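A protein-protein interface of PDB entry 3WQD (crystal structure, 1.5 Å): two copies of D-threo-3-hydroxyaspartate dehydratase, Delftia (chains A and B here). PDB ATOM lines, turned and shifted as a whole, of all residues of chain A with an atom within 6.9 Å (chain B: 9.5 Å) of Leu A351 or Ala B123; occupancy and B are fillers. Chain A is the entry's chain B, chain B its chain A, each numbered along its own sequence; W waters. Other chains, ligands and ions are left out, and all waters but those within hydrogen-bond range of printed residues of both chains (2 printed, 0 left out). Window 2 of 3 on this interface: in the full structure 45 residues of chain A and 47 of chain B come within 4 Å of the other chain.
No position is printed for both chains.
Water W2 bridges O of Ile A275 (2.7 Å) and O of Met B97 (2.7 Å). Water W1 lies within hydrogen-bond range of the side-chain carboxylate of Asp B120 (2.9 Å) and the backbone NH of His A277 (3.0 Å).
The guanidinium group of Arg B101 is in hydrogen-bond range of a ring nitrogen (NE2) of His B100 (3.4 Å). The side-chain hydroxyl (OG) of Ser B121 lies within hydrogen-bond range of the backbone NH (N) of Ala B124, at 3.1 Å. The backbone carbonyl oxygen (O) of Ile A285 lies within hydrogen-bond range of the backbone NH (N) of Ile A275 (2.8 Å).
Printed residues of chain B within 4 Å of Thr A273: His B100. Of the printed residues of chain B, Ile A275 touches Ser B96 and Ala B98. No residue of chain B comes within 4 Å of Pro A350. Leu A351 touches just these residues of chain B: Ala B123 (3.8 Å) and Ala B124 (3.7 Å). Of the printed residues of chain A, Ser B96 touches Ile A275. Printed residues of chain A within 4 Å of Ala B98: Ile A275. Asp B120 touches none of the printed residues of chain A. Printed residues of chain A within 4 Å of Ala B123: Leu A351. Of the printed residues of chain A, Ala B124 touches Leu A351 (3.7 Å). Ile B128 touches none of the printed residues of chain A.
His B100 touches Thr A273. Ser B96 touches Ile A275. Ile A275 touches Ala B98 (CG2 to CB, 3.9 Å). CD2 of Leu A351 touches CB of Ala B123 (3.8 Å). CD2 of Leu A351 touches N of Ala B124, at 3.7 Å. Arg A354 touches His B100.
Along chain B the printed residues that touch a printed residue of chain A span positions 96 to 124. Of the 13 printed residues of chain A, 4 touch a printed residue of chain B. Printed residues of chain A that touch a printed residue of chain B: Thr A273, Ile A275, Leu A351 and Arg A354.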
ATOM      1  N   THR A 273      -9.510 -26.696 -16.774  1.00  0.00           N
ATOM      2  CA  THR A 273      -8.298 -26.240 -17.430  1.00  0.00           C
ATOM      3  C   THR A 273      -7.479 -27.429 -17.938  1.00  0.00           C
ATOM      4  O   THR A 273      -7.349 -28.433 -17.200  1.00  0.00           O
ATOM      5  CB  THR A 273      -7.401 -25.411 -16.394  1.00  0.00           C
ATOM      6  OG1 THR A 273      -8.144 -24.250 -16.014  1.00  0.00           O
ATOM      7  CG2 THR A 273      -6.081 -24.901 -17.044  1.00  0.00           C
ATOM      8  N   VAL A 274      -6.833 -27.282 -19.140  1.00  0.00           N
ATOM      9  CA  VAL A 274      -5.876 -28.272 -19.606  1.00  0.00           C
ATOM     10  C   VAL A 274      -4.569 -28.138 -18.830  1.00  0.00           C
ATOM     11  O   VAL A 274      -3.968 -27.028 -18.798  1.00  0.00           O
ATOM     12  CB  VAL A 274      -5.627 -28.066 -21.119  1.00  0.00           C
ATOM     13  CG1 VAL A 274      -4.562 -29.102 -21.571  1.00  0.00           C
ATOM     14  CG2 VAL A 274      -6.958 -28.288 -21.897  1.00  0.00           C
ATOM     15  N   ILE A 275      -4.154 -29.202 -18.150  1.00  0.00           N
ATOM     16  CA  ILE A 275      -2.950 -29.209 -17.337  1.00  0.00           C
ATOM     17  C   ILE A 275      -1.816 -30.135 -17.831  1.00  0.00           C
ATOM     18  O   ILE A 275      -0.704 -30.156 -17.262  1.00  0.00           O
ATOM     19  CB  ILE A 275      -3.282 -29.548 -15.862  1.00  0.00           C
ATOM     20  CG1 ILE A 275      -3.881 -30.978 -15.803  1.00  0.00           C
ATOM     21  CG2 ILE A 275      -4.217 -28.498 -15.216  1.00  0.00           C
ATOM     22  CD1 ILE A 275      -4.111 -31.501 -14.375  1.00  0.00           C
ATOM     23  N   GLY A 276      -2.043 -30.817 -18.946  1.00  0.00           N
ATOM     24  CA  GLY A 276      -1.014 -31.709 -19.487  1.00  0.00           C
ATOM     25  C   GLY A 276      -1.513 -32.438 -20.697  1.00  0.00           C
ATOM     26  O   GLY A 276      -2.658 -32.226 -21.143  1.00  0.00           O
ATOM     27  N   HIS A 277      -0.630 -33.284 -21.251  1.00  0.00           N
ATOM     28  CA  HIS A 277      -0.907 -34.119 -22.405  1.00  0.00           C
ATOM     29  C   HIS A 277      -0.201 -35.464 -22.318  1.00  0.00           C
ATOM     30  O   HIS A 277       0.847 -35.595 -21.660  1.00  0.00           O
ATOM     31  CB  HIS A 277      -0.451 -33.429 -23.700  1.00  0.00           C
ATOM     32  CG  HIS A 277      -1.112 -32.070 -23.910  1.00  0.00           C
ATOM     33  ND1 HIS A 277      -0.560 -30.885 -23.465  1.00  0.00           N
ATOM     34  CD2 HIS A 277      -2.331 -31.733 -24.489  1.00  0.00           C
ATOM     35  CE1 HIS A 277      -1.391 -29.862 -23.744  1.00  0.00           C
ATOM     36  NE2 HIS A 277      -2.477 -30.377 -24.378  1.00  0.00           N
ATOM     37  N   ILE A 285      -4.954 -33.763 -20.682  1.00  0.00           N
ATOM     38  CA  ILE A 285      -5.296 -33.991 -19.285  1.00  0.00           C
ATOM     39  C   ILE A 285      -5.914 -32.711 -18.751  1.00  0.00           C
ATOM     40  O   ILE A 285      -5.304 -31.609 -18.920  1.00  0.00           O
ATOM     41  CB  ILE A 285      -4.047 -34.364 -18.419  1.00  0.00           C
ATOM     42  CG1 ILE A 285      -3.148 -35.476 -19.032  1.00  0.00           C
ATOM     43  CG2 ILE A 285      -4.511 -34.668 -16.971  1.00  0.00           C
ATOM     44  CD1 ILE A 285      -3.826 -36.718 -19.392  1.00  0.00           C
ATOM     45  N   ALA A 346      -1.691 -31.313 -28.361  1.00  0.00           N
ATOM     46  CA  ALA A 346      -1.216 -30.101 -27.619  1.00  0.00           C
ATOM     47  C   ALA A 346      -1.508 -28.803 -28.398  1.00  0.00           C
ATOM     48  O   ALA A 346      -1.665 -27.739 -27.806  1.00  0.00           O
ATOM     49  CB  ALA A 346       0.280 -30.204 -27.238  1.00  0.00           C
ATOM     50  N   PHE A 349      -5.438 -28.505 -28.018  1.00  0.00           N
ATOM     51  CA  PHE A 349      -5.792 -28.147 -26.636  1.00  0.00           C
ATOM     52  C   PHE A 349      -4.557 -27.678 -25.872  1.00  0.00           C
ATOM     53  O   PHE A 349      -4.038 -28.450 -25.043  1.00  0.00           O
ATOM     54  CB  PHE A 349      -6.470 -29.377 -25.904  1.00  0.00           C
ATOM     55  CG  PHE A 349      -7.797 -29.733 -26.497  1.00  0.00           C
ATOM     56  CD1 PHE A 349      -8.980 -28.962 -26.179  1.00  0.00           C
ATOM     57  CD2 PHE A 349      -7.915 -30.830 -27.405  1.00  0.00           C
ATOM     58  CE1 PHE A 349     -10.221 -29.301 -26.766  1.00  0.00           C
ATOM     59  CE2 PHE A 349      -9.153 -31.140 -28.004  1.00  0.00           C
ATOM     60  CZ  PHE A 349     -10.304 -30.397 -27.682  1.00  0.00           C
ATOM     61  N   PRO A 350      -4.103 -26.426 -26.095  1.00  0.00           N
ATOM     62  CA  PRO A 350      -2.870 -25.942 -25.416  1.00  0.00           C
ATOM     63  C   PRO A 350      -2.920 -25.903 -23.865  1.00  0.00           C
ATOM     64  O   PRO A 350      -3.990 -25.678 -23.265  1.00  0.00           O
ATOM     65  CB  PRO A 350      -2.661 -24.509 -26.015  1.00  0.00           C
ATOM     66  CG  PRO A 350      -3.430 -24.541 -27.300  1.00  0.00           C
ATOM     67  CD  PRO A 350      -4.627 -25.440 -27.051  1.00  0.00           C
ATOM     68  N   LEU A 351      -1.806 -26.260 -23.204  1.00  0.00           N
ATOM     69  CA  LEU A 351      -1.695 -26.069 -21.774  1.00  0.00           C
ATOM     70  C   LEU A 351      -2.357 -24.732 -21.347  1.00  0.00           C
ATOM     71  O   LEU A 351      -2.147 -23.716 -22.006  1.00  0.00           O
ATOM     72  CB  LEU A 351      -0.191 -26.116 -21.329  1.00  0.00           C
ATOM     73  CG  LEU A 351       0.118 -25.842 -19.796  1.00  0.00           C
ATOM     74  CD1 LEU A 351      -0.253 -27.053 -18.956  1.00  0.00           C
ATOM     75  CD2 LEU A 351       1.602 -25.419 -19.551  1.00  0.00           C
ATOM     76  N   GLY A 352      -3.230 -24.769 -20.320  1.00  0.00           N
ATOM     77  CA  GLY A 352      -3.862 -23.537 -19.800  1.00  0.00           C
ATOM     78  C   GLY A 352      -5.169 -23.253 -20.481  1.00  0.00           C
ATOM     79  O   GLY A 352      -5.915 -22.434 -19.988  1.00  0.00           O
ATOM     80  N   THR A 353      -5.509 -23.976 -21.575  1.00  0.00           N
ATOM     81  CA  THR A 353      -6.812 -23.760 -22.288  1.00  0.00           C
ATOM     82  C   THR A 353      -7.975 -24.051 -21.335  1.00  0.00           C
ATOM     83  O   THR A 353      -7.880 -25.056 -20.619  1.00  0.00           O
ATOM     84  CB  THR A 353      -6.999 -24.706 -23.519  1.00  0.00           C
ATOM     85  OG1 THR A 353      -5.964 -24.507 -24.427  1.00  0.00           O
ATOM     86  CG2 THR A 353      -8.370 -24.520 -24.276  1.00  0.00           C
ATOM     87  N   ARG A 354      -9.040 -23.224 -21.364  1.00  0.00           N
ATOM     88  CA  ARG A 354     -10.224 -23.538 -20.538  1.00  0.00           C
ATOM     89  C   ARG A 354     -11.287 -24.123 -21.435  1.00  0.00           C
ATOM     90  O   ARG A 354     -11.530 -23.619 -22.559  1.00  0.00           O
ATOM     91  CB  ARG A 354     -10.767 -22.286 -19.841  1.00  0.00           C
ATOM     92  CG  ARG A 354      -9.790 -21.746 -18.815  1.00  0.00           C
ATOM     93  CD  ARG A 354     -10.207 -20.466 -18.141  1.00  0.00           C
ATOM     94  NE  ARG A 354      -9.260 -20.344 -17.020  1.00  0.00           N
ATOM     95  CZ  ARG A 354      -9.601 -20.119 -15.756  1.00  0.00           C
ATOM     96  NH1 ARG A 354     -10.829 -19.732 -15.468  1.00  0.00           N
ATOM     97  NH2 ARG A 354      -8.666 -20.137 -14.807  1.00  0.00           N
ATOM     98  N   SER B  96      -0.314 -32.201 -11.850  1.00  0.00           N
ATOM     99  CA  SER B  96       0.374 -31.301 -12.734  1.00  0.00           C
ATOM    100  C   SER B  96      -0.027 -29.886 -12.513  1.00  0.00           C
ATOM    101  O   SER B  96      -1.242 -29.569 -12.670  1.00  0.00           O
ATOM    102  CB  SER B  96       0.025 -31.622 -14.158  1.00  0.00           C
ATOM    103  OG  SER B  96       1.073 -32.152 -14.716  1.00  0.00           O
ATOM    104  N   MET B  97       0.987 -29.004 -12.288  1.00  0.00           N
ATOM    105  CA  MET B  97       0.670 -27.631 -11.891  1.00  0.00           C
ATOM    106  C   MET B  97       0.056 -26.806 -13.052  1.00  0.00           C
ATOM    107  O   MET B  97       0.624 -26.754 -14.174  1.00  0.00           O
ATOM    108  CB  MET B  97       1.932 -26.957 -11.329  1.00  0.00           C
ATOM    109  CG  MET B  97       1.690 -25.510 -10.950  1.00  0.00           C
ATOM    110  SD  MET B  97       0.545 -25.530  -9.507  1.00  0.00           S
ATOM    111  CE  MET B  97       0.461 -23.725  -9.133  1.00  0.00           C
ATOM    112  N   ALA B  98      -1.097 -26.166 -12.820  1.00  0.00           N
ATOM    113  CA  ALA B  98      -1.676 -25.229 -13.731  1.00  0.00           C
ATOM    114  C   ALA B  98      -1.103 -23.806 -13.457  1.00  0.00           C
ATOM    115  O   ALA B  98      -1.170 -23.316 -12.334  1.00  0.00           O
ATOM    116  CB  ALA B  98      -3.160 -25.195 -13.489  1.00  0.00           C
ATOM    117  N   PRO B  99      -0.551 -23.163 -14.509  1.00  0.00           N
ATOM    118  CA  PRO B  99       0.097 -21.856 -14.267  1.00  0.00           C
ATOM    119  C   PRO B  99      -0.853 -20.829 -13.580  1.00  0.00           C
ATOM    120  O   PRO B  99      -0.414 -20.023 -12.779  1.00  0.00           O
ATOM    121  CB  PRO B  99       0.566 -21.437 -15.697  1.00  0.00           C
ATOM    122  CG  PRO B  99       0.892 -22.751 -16.353  1.00  0.00           C
ATOM    123  CD  PRO B  99      -0.211 -23.671 -15.867  1.00  0.00           C
ATOM    124  N   HIS B 100      -2.163 -20.897 -13.883  1.00  0.00           N
ATOM    125  CA  HIS B 100      -3.069 -19.914 -13.281  1.00  0.00           C
ATOM    126  C   HIS B 100      -3.135 -20.052 -11.748  1.00  0.00           C
ATOM    127  O   HIS B 100      -3.572 -19.100 -11.094  1.00  0.00           O
ATOM    128  CB  HIS B 100      -4.436 -19.907 -13.957  1.00  0.00           C
ATOM    129  CG  HIS B 100      -5.339 -20.975 -13.492  1.00  0.00           C
ATOM    130  ND1 HIS B 100      -5.444 -22.182 -14.143  1.00  0.00           N
ATOM    131  CD2 HIS B 100      -6.184 -21.032 -12.399  1.00  0.00           C
ATOM    132  CE1 HIS B 100      -6.332 -22.971 -13.494  1.00  0.00           C
ATOM    133  NE2 HIS B 100      -6.792 -22.281 -12.419  1.00  0.00           N
ATOM    134  N   ARG B 101      -2.797 -21.224 -11.183  1.00  0.00           N
ATOM    135  CA  ARG B 101      -2.776 -21.364  -9.722  1.00  0.00           C
ATOM    136  C   ARG B 101      -1.451 -20.932  -9.068  1.00  0.00           C
ATOM    137  O   ARG B 101      -1.305 -21.017  -7.839  1.00  0.00           O
ATOM    138  CB  ARG B 101      -3.054 -22.838  -9.368  1.00  0.00           C
ATOM    139  CG  ARG B 101      -4.548 -23.183  -9.498  1.00  0.00           C
ATOM    140  CD  ARG B 101      -4.840 -24.592  -8.942  1.00  0.00           C
ATOM    141  NE  ARG B 101      -4.775 -25.653  -9.974  1.00  0.00           N
ATOM    142  CZ  ARG B 101      -5.781 -25.993 -10.787  1.00  0.00           C
ATOM    143  NH1 ARG B 101      -6.905 -25.291 -10.849  1.00  0.00           N
ATOM    144  NH2 ARG B 101      -5.607 -26.992 -11.638  1.00  0.00           N
ATOM    145  N   LEU B 102      -0.518 -20.378  -9.862  1.00  0.00           N
ATOM    146  CA  LEU B 102       0.778 -19.985  -9.280  1.00  0.00           C
ATOM    147  C   LEU B 102       0.613 -18.896  -8.182  1.00  0.00           C
ATOM    148  O   LEU B 102       1.301 -18.972  -7.175  1.00  0.00           O
ATOM    149  CB  LEU B 102       1.775 -19.606 -10.367  1.00  0.00           C
ATOM    150  CG  LEU B 102       2.479 -20.859 -10.962  1.00  0.00           C
ATOM    151  CD1 LEU B 102       3.123 -20.456 -12.297  1.00  0.00           C
ATOM    152  CD2 LEU B 102       3.543 -21.438 -10.004  1.00  0.00           C
ATOM    153  N   ILE B 118       4.494 -30.190  -8.911  1.00  0.00           N
ATOM    154  CA  ILE B 118       4.973 -31.143  -9.904  1.00  0.00           C
ATOM    155  C   ILE B 118       4.637 -30.695 -11.310  1.00  0.00           C
ATOM    156  O   ILE B 118       3.650 -29.971 -11.584  1.00  0.00           O
ATOM    157  CB  ILE B 118       4.438 -32.600  -9.646  1.00  0.00           C
ATOM    158  CG1 ILE B 118       2.963 -32.763 -10.107  1.00  0.00           C
ATOM    159  CG2 ILE B 118       4.522 -32.962  -8.146  1.00  0.00           C
ATOM    160  CD1 ILE B 118       2.441 -34.226  -9.934  1.00  0.00           C
ATOM    161  N   VAL B 119       5.501 -31.146 -12.243  1.00  0.00           N
ATOM    162  CA  VAL B 119       5.250 -30.814 -13.662  1.00  0.00           C
ATOM    163  C   VAL B 119       5.722 -32.012 -14.505  1.00  0.00           C
ATOM    164  O   VAL B 119       6.514 -32.864 -14.058  1.00  0.00           O
ATOM    165  CB  VAL B 119       6.046 -29.558 -14.166  1.00  0.00           C
ATOM    166  CG1 VAL B 119       5.616 -28.254 -13.410  1.00  0.00           C
ATOM    167  CG2 VAL B 119       7.588 -29.772 -14.071  1.00  0.00           C
ATOM    168  N   ASP B 120       5.301 -32.021 -15.762  1.00  0.00           N
ATOM    169  CA  ASP B 120       5.741 -33.091 -16.694  1.00  0.00           C
ATOM    170  C   ASP B 120       5.955 -32.508 -18.093  1.00  0.00           C
ATOM    171  O   ASP B 120       6.038 -33.268 -19.084  1.00  0.00           O
ATOM    172  CB  ASP B 120       4.739 -34.267 -16.728  1.00  0.00           C
ATOM    173  CG  ASP B 120       3.440 -33.920 -17.376  1.00  0.00           C
ATOM    174  OD1 ASP B 120       3.203 -32.731 -17.746  1.00  0.00           O
ATOM    175  OD2 ASP B 120       2.608 -34.836 -17.570  1.00  0.00           O
ATOM    176  N   SER B 121       6.132 -31.163 -18.203  1.00  0.00           N
ATOM    177  CA  SER B 121       6.255 -30.527 -19.535  1.00  0.00           C
ATOM    178  C   SER B 121       7.239 -29.358 -19.383  1.00  0.00           C
ATOM    179  O   SER B 121       7.358 -28.725 -18.302  1.00  0.00           O
ATOM    180  CB  SER B 121       4.878 -30.071 -20.106  1.00  0.00           C
ATOM    181  OG  SER B 121       4.379 -28.952 -19.395  1.00  0.00           O
ATOM    182  N   VAL B 122       7.968 -29.075 -20.447  1.00  0.00           N
ATOM    183  CA  VAL B 122       8.766 -27.855 -20.541  1.00  0.00           C
ATOM    184  C   VAL B 122       7.921 -26.609 -20.348  1.00  0.00           C
ATOM    185  O   VAL B 122       8.373 -25.734 -19.598  1.00  0.00           O
ATOM    186  CB  VAL B 122       9.612 -27.857 -21.848  1.00  0.00           C
ATOM    187  CG1 VAL B 122      10.268 -26.489 -22.063  1.00  0.00           C
ATOM    188  CG2 VAL B 122      10.687 -28.947 -21.792  1.00  0.00           C
ATOM    189  N   ALA B 123       6.767 -26.456 -21.016  1.00  0.00           N
ATOM    190  CA  ALA B 123       5.986 -25.213 -20.868  1.00  0.00           C
ATOM    191  C   ALA B 123       5.564 -24.975 -19.402  1.00  0.00           C
ATOM    192  O   ALA B 123       5.600 -23.800 -18.911  1.00  0.00           O
ATOM    193  CB  ALA B 123       4.737 -25.250 -21.755  1.00  0.00           C
ATOM    194  N   ALA B 124       5.131 -26.035 -18.691  1.00  0.00           N
ATOM    195  CA  ALA B 124       4.717 -25.814 -17.305  1.00  0.00           C
ATOM    196  C   ALA B 124       5.955 -25.434 -16.451  1.00  0.00           C
ATOM    197  O   ALA B 124       5.852 -24.559 -15.564  1.00  0.00           O
ATOM    198  CB  ALA B 124       4.052 -27.076 -16.734  1.00  0.00           C
ATOM    199  N   ALA B 125       7.112 -26.083 -16.693  1.00  0.00           N
ATOM    200  CA  ALA B 125       8.328 -25.745 -15.960  1.00  0.00           C
ATOM    201  C   ALA B 125       8.760 -24.275 -16.229  1.00  0.00           C
ATOM    202  O   ALA B 125       9.131 -23.536 -15.258  1.00  0.00           O
ATOM    203  CB  ALA B 125       9.463 -26.688 -16.307  1.00  0.00           C
ATOM    204  N   GLN B 126       8.601 -23.813 -17.494  1.00  0.00           N
ATOM    205  CA  GLN B 126       8.972 -22.417 -17.844  1.00  0.00           C
ATOM    206  C   GLN B 126       8.062 -21.440 -17.157  1.00  0.00           C
ATOM    207  O   GLN B 126       8.511 -20.345 -16.732  1.00  0.00           O
ATOM    208  CB  GLN B 126       8.918 -22.192 -19.352  1.00  0.00           C
ATOM    209  CG  GLN B 126       9.963 -23.002 -20.151  1.00  0.00           C
ATOM    210  CD  GLN B 126       9.799 -22.857 -21.668  1.00  0.00           C
ATOM    211  OE1 GLN B 126       8.681 -22.902 -22.208  1.00  0.00           O
ATOM    212  NE2 GLN B 126      10.911 -22.729 -22.370  1.00  0.00           N
ATOM    213  N   ALA B 127       6.772 -21.801 -17.071  1.00  0.00           N
ATOM    214  CA  ALA B 127       5.773 -20.854 -16.457  1.00  0.00           C
ATOM    215  C   ALA B 127       6.150 -20.680 -14.961  1.00  0.00           C
ATOM    216  O   ALA B 127       6.109 -19.551 -14.418  1.00  0.00           O
ATOM    217  CB  ALA B 127       4.339 -21.311 -16.608  1.00  0.00           C
ATOM    218  N   ILE B 128       6.429 -21.799 -14.274  1.00  0.00           N
ATOM    219  CA  ILE B 128       6.828 -21.723 -12.846  1.00  0.00           C
ATOM    220  C   ILE B 128       8.117 -20.926 -12.665  1.00  0.00           C
ATOM    221  O   ILE B 128       8.143 -19.981 -11.848  1.00  0.00           O
ATOM    222  CB  ILE B 128       7.004 -23.118 -12.214  1.00  0.00           C
ATOM    223  CG1 ILE B 128       5.660 -23.878 -12.257  1.00  0.00           C
ATOM    224  CG2 ILE B 128       7.464 -22.946 -10.743  1.00  0.00           C
ATOM    225  CD1 ILE B 128       5.729 -25.331 -11.695  1.00  0.00           C
ATOM    226  N   ALA B 129       9.141 -21.289 -13.456  1.00  0.00           N
ATOM    227  CA  ALA B 129      10.461 -20.626 -13.281  1.00  0.00           C
ATOM    228  C   ALA B 129      10.384 -19.108 -13.576  1.00  0.00           C
ATOM    229  O   ALA B 129      10.892 -18.301 -12.737  1.00  0.00           O
ATOM    230  CB  ALA B 129      11.506 -21.314 -14.117  1.00  0.00           C
ATOM    231  N   ALA B 130       9.650 -18.701 -14.609  1.00  0.00           N
ATOM    232  CA  ALA B 130       9.526 -17.273 -14.932  1.00  0.00           C
ATOM    233  C   ALA B 130       8.761 -16.537 -13.818  1.00  0.00           C
ATOM    234  O   ALA B 130       9.189 -15.459 -13.300  1.00  0.00           O
ATOM    235  CB  ALA B 130       8.871 -17.059 -16.297  1.00  0.00           C
ATOM    236  N   PHE B 131       7.666 -17.137 -13.330  1.00  0.00           N
ATOM    237  CA  PHE B 131       6.931 -16.459 -12.246  1.00  0.00           C
ATOM    238  C   PHE B 131       7.788 -16.393 -11.006  1.00  0.00           C
ATOM    239  O   PHE B 131       7.755 -15.394 -10.279  1.00  0.00           O
ATOM    240  CB  PHE B 131       5.618 -17.236 -11.977  1.00  0.00           C
ATOM    241  CG  PHE B 131       4.695 -16.530 -11.028  1.00  0.00           C
ATOM    242  CD1 PHE B 131       4.071 -15.301 -11.362  1.00  0.00           C
ATOM    243  CD2 PHE B 131       4.387 -17.123  -9.783  1.00  0.00           C
ATOM    244  CE1 PHE B 131       3.226 -14.634 -10.470  1.00  0.00           C
ATOM    245  CE2 PHE B 131       3.487 -16.473  -8.894  1.00  0.00           C
ATOM    246  CZ  PHE B 131       2.908 -15.267  -9.248  1.00  0.00           C
ATOM    247  N   LEU B 161      13.317 -35.317 -22.851  1.00  0.00           N
ATOM    248  CA  LEU B 161      12.252 -34.541 -22.212  1.00  0.00           C
ATOM    249  C   LEU B 161      12.554 -34.346 -20.704  1.00  0.00           C
ATOM    250  O   LEU B 161      12.466 -33.195 -20.154  1.00  0.00           O
ATOM    251  CB  LEU B 161      10.855 -35.140 -22.398  1.00  0.00           C
ATOM    252  CG  LEU B 161       9.712 -34.384 -21.679  1.00  0.00           C
ATOM    253  CD1 LEU B 161       9.647 -32.901 -22.042  1.00  0.00           C
ATOM    254  CD2 LEU B 161       8.370 -35.085 -21.934  1.00  0.00           C
ATOM    255  N   ALA B 164      15.333 -31.833 -20.365  1.00  0.00           N
ATOM    256  CA  ALA B 164      14.909 -30.487 -20.782  1.00  0.00           C
ATOM    257  C   ALA B 164      14.128 -29.844 -19.644  1.00  0.00           C
ATOM    258  O   ALA B 164      14.308 -28.609 -19.349  1.00  0.00           O
ATOM    259  CB  ALA B 164      14.089 -30.504 -22.063  1.00  0.00           C
ATOM    260  N   ILE B 165      13.245 -30.608 -18.972  1.00  0.00           N
ATOM    261  CA  ILE B 165      12.438 -30.036 -17.879  1.00  0.00           C
ATOM    262  C   ILE B 165      13.373 -29.795 -16.676  1.00  0.00           C
ATOM    263  O   ILE B 165      13.322 -28.683 -16.055  1.00  0.00           O
ATOM    264  CB  ILE B 165      11.306 -31.007 -17.441  1.00  0.00           C
ATOM    265  CG1 ILE B 165      10.339 -31.257 -18.592  1.00  0.00           C
ATOM    266  CG2 ILE B 165      10.645 -30.492 -16.102  1.00  0.00           C
ATOM    267  CD1 ILE B 165       9.495 -32.492 -18.364  1.00  0.00           C
ATOM    268  N   THR B 168      15.342 -26.664 -17.309  1.00  0.00           N
ATOM    269  CA  THR B 168      14.493 -25.477 -17.215  1.00  0.00           C
ATOM    270  C   THR B 168      14.332 -25.025 -15.746  1.00  0.00           C
ATOM    271  O   THR B 168      14.405 -23.823 -15.447  1.00  0.00           O
ATOM    272  CB  THR B 168      13.115 -25.752 -17.850  1.00  0.00           C
ATOM    273  OG1 THR B 168      13.317 -26.055 -19.219  1.00  0.00           O
ATOM    274  CG2 THR B 168      12.181 -24.526 -17.775  1.00  0.00           C
ATOM    275  N   LEU B 169      14.038 -25.982 -14.878  1.00  0.00           N
ATOM    276  CA  LEU B 169      13.839 -25.654 -13.478  1.00  0.00           C
ATOM    277  C   LEU B 169      15.140 -25.225 -12.842  1.00  0.00           C
ATOM    278  O   LEU B 169      15.194 -24.180 -12.192  1.00  0.00           O
ATOM    279  CB  LEU B 169      13.264 -26.850 -12.738  1.00  0.00           C
ATOM    280  CG  LEU B 169      11.832 -27.332 -13.147  1.00  0.00           C
ATOM    281  CD1 LEU B 169      11.549 -28.740 -12.610  1.00  0.00           C
ATOM    282  CD2 LEU B 169      10.878 -26.267 -12.644  1.00  0.00           C
HETATM  283  O   HOH W   1       2.175 -32.651 -20.437  1.00  0.00           O
HETATM  284  O   HOH W   2       1.142 -28.735 -15.978  1.00  0.00           O
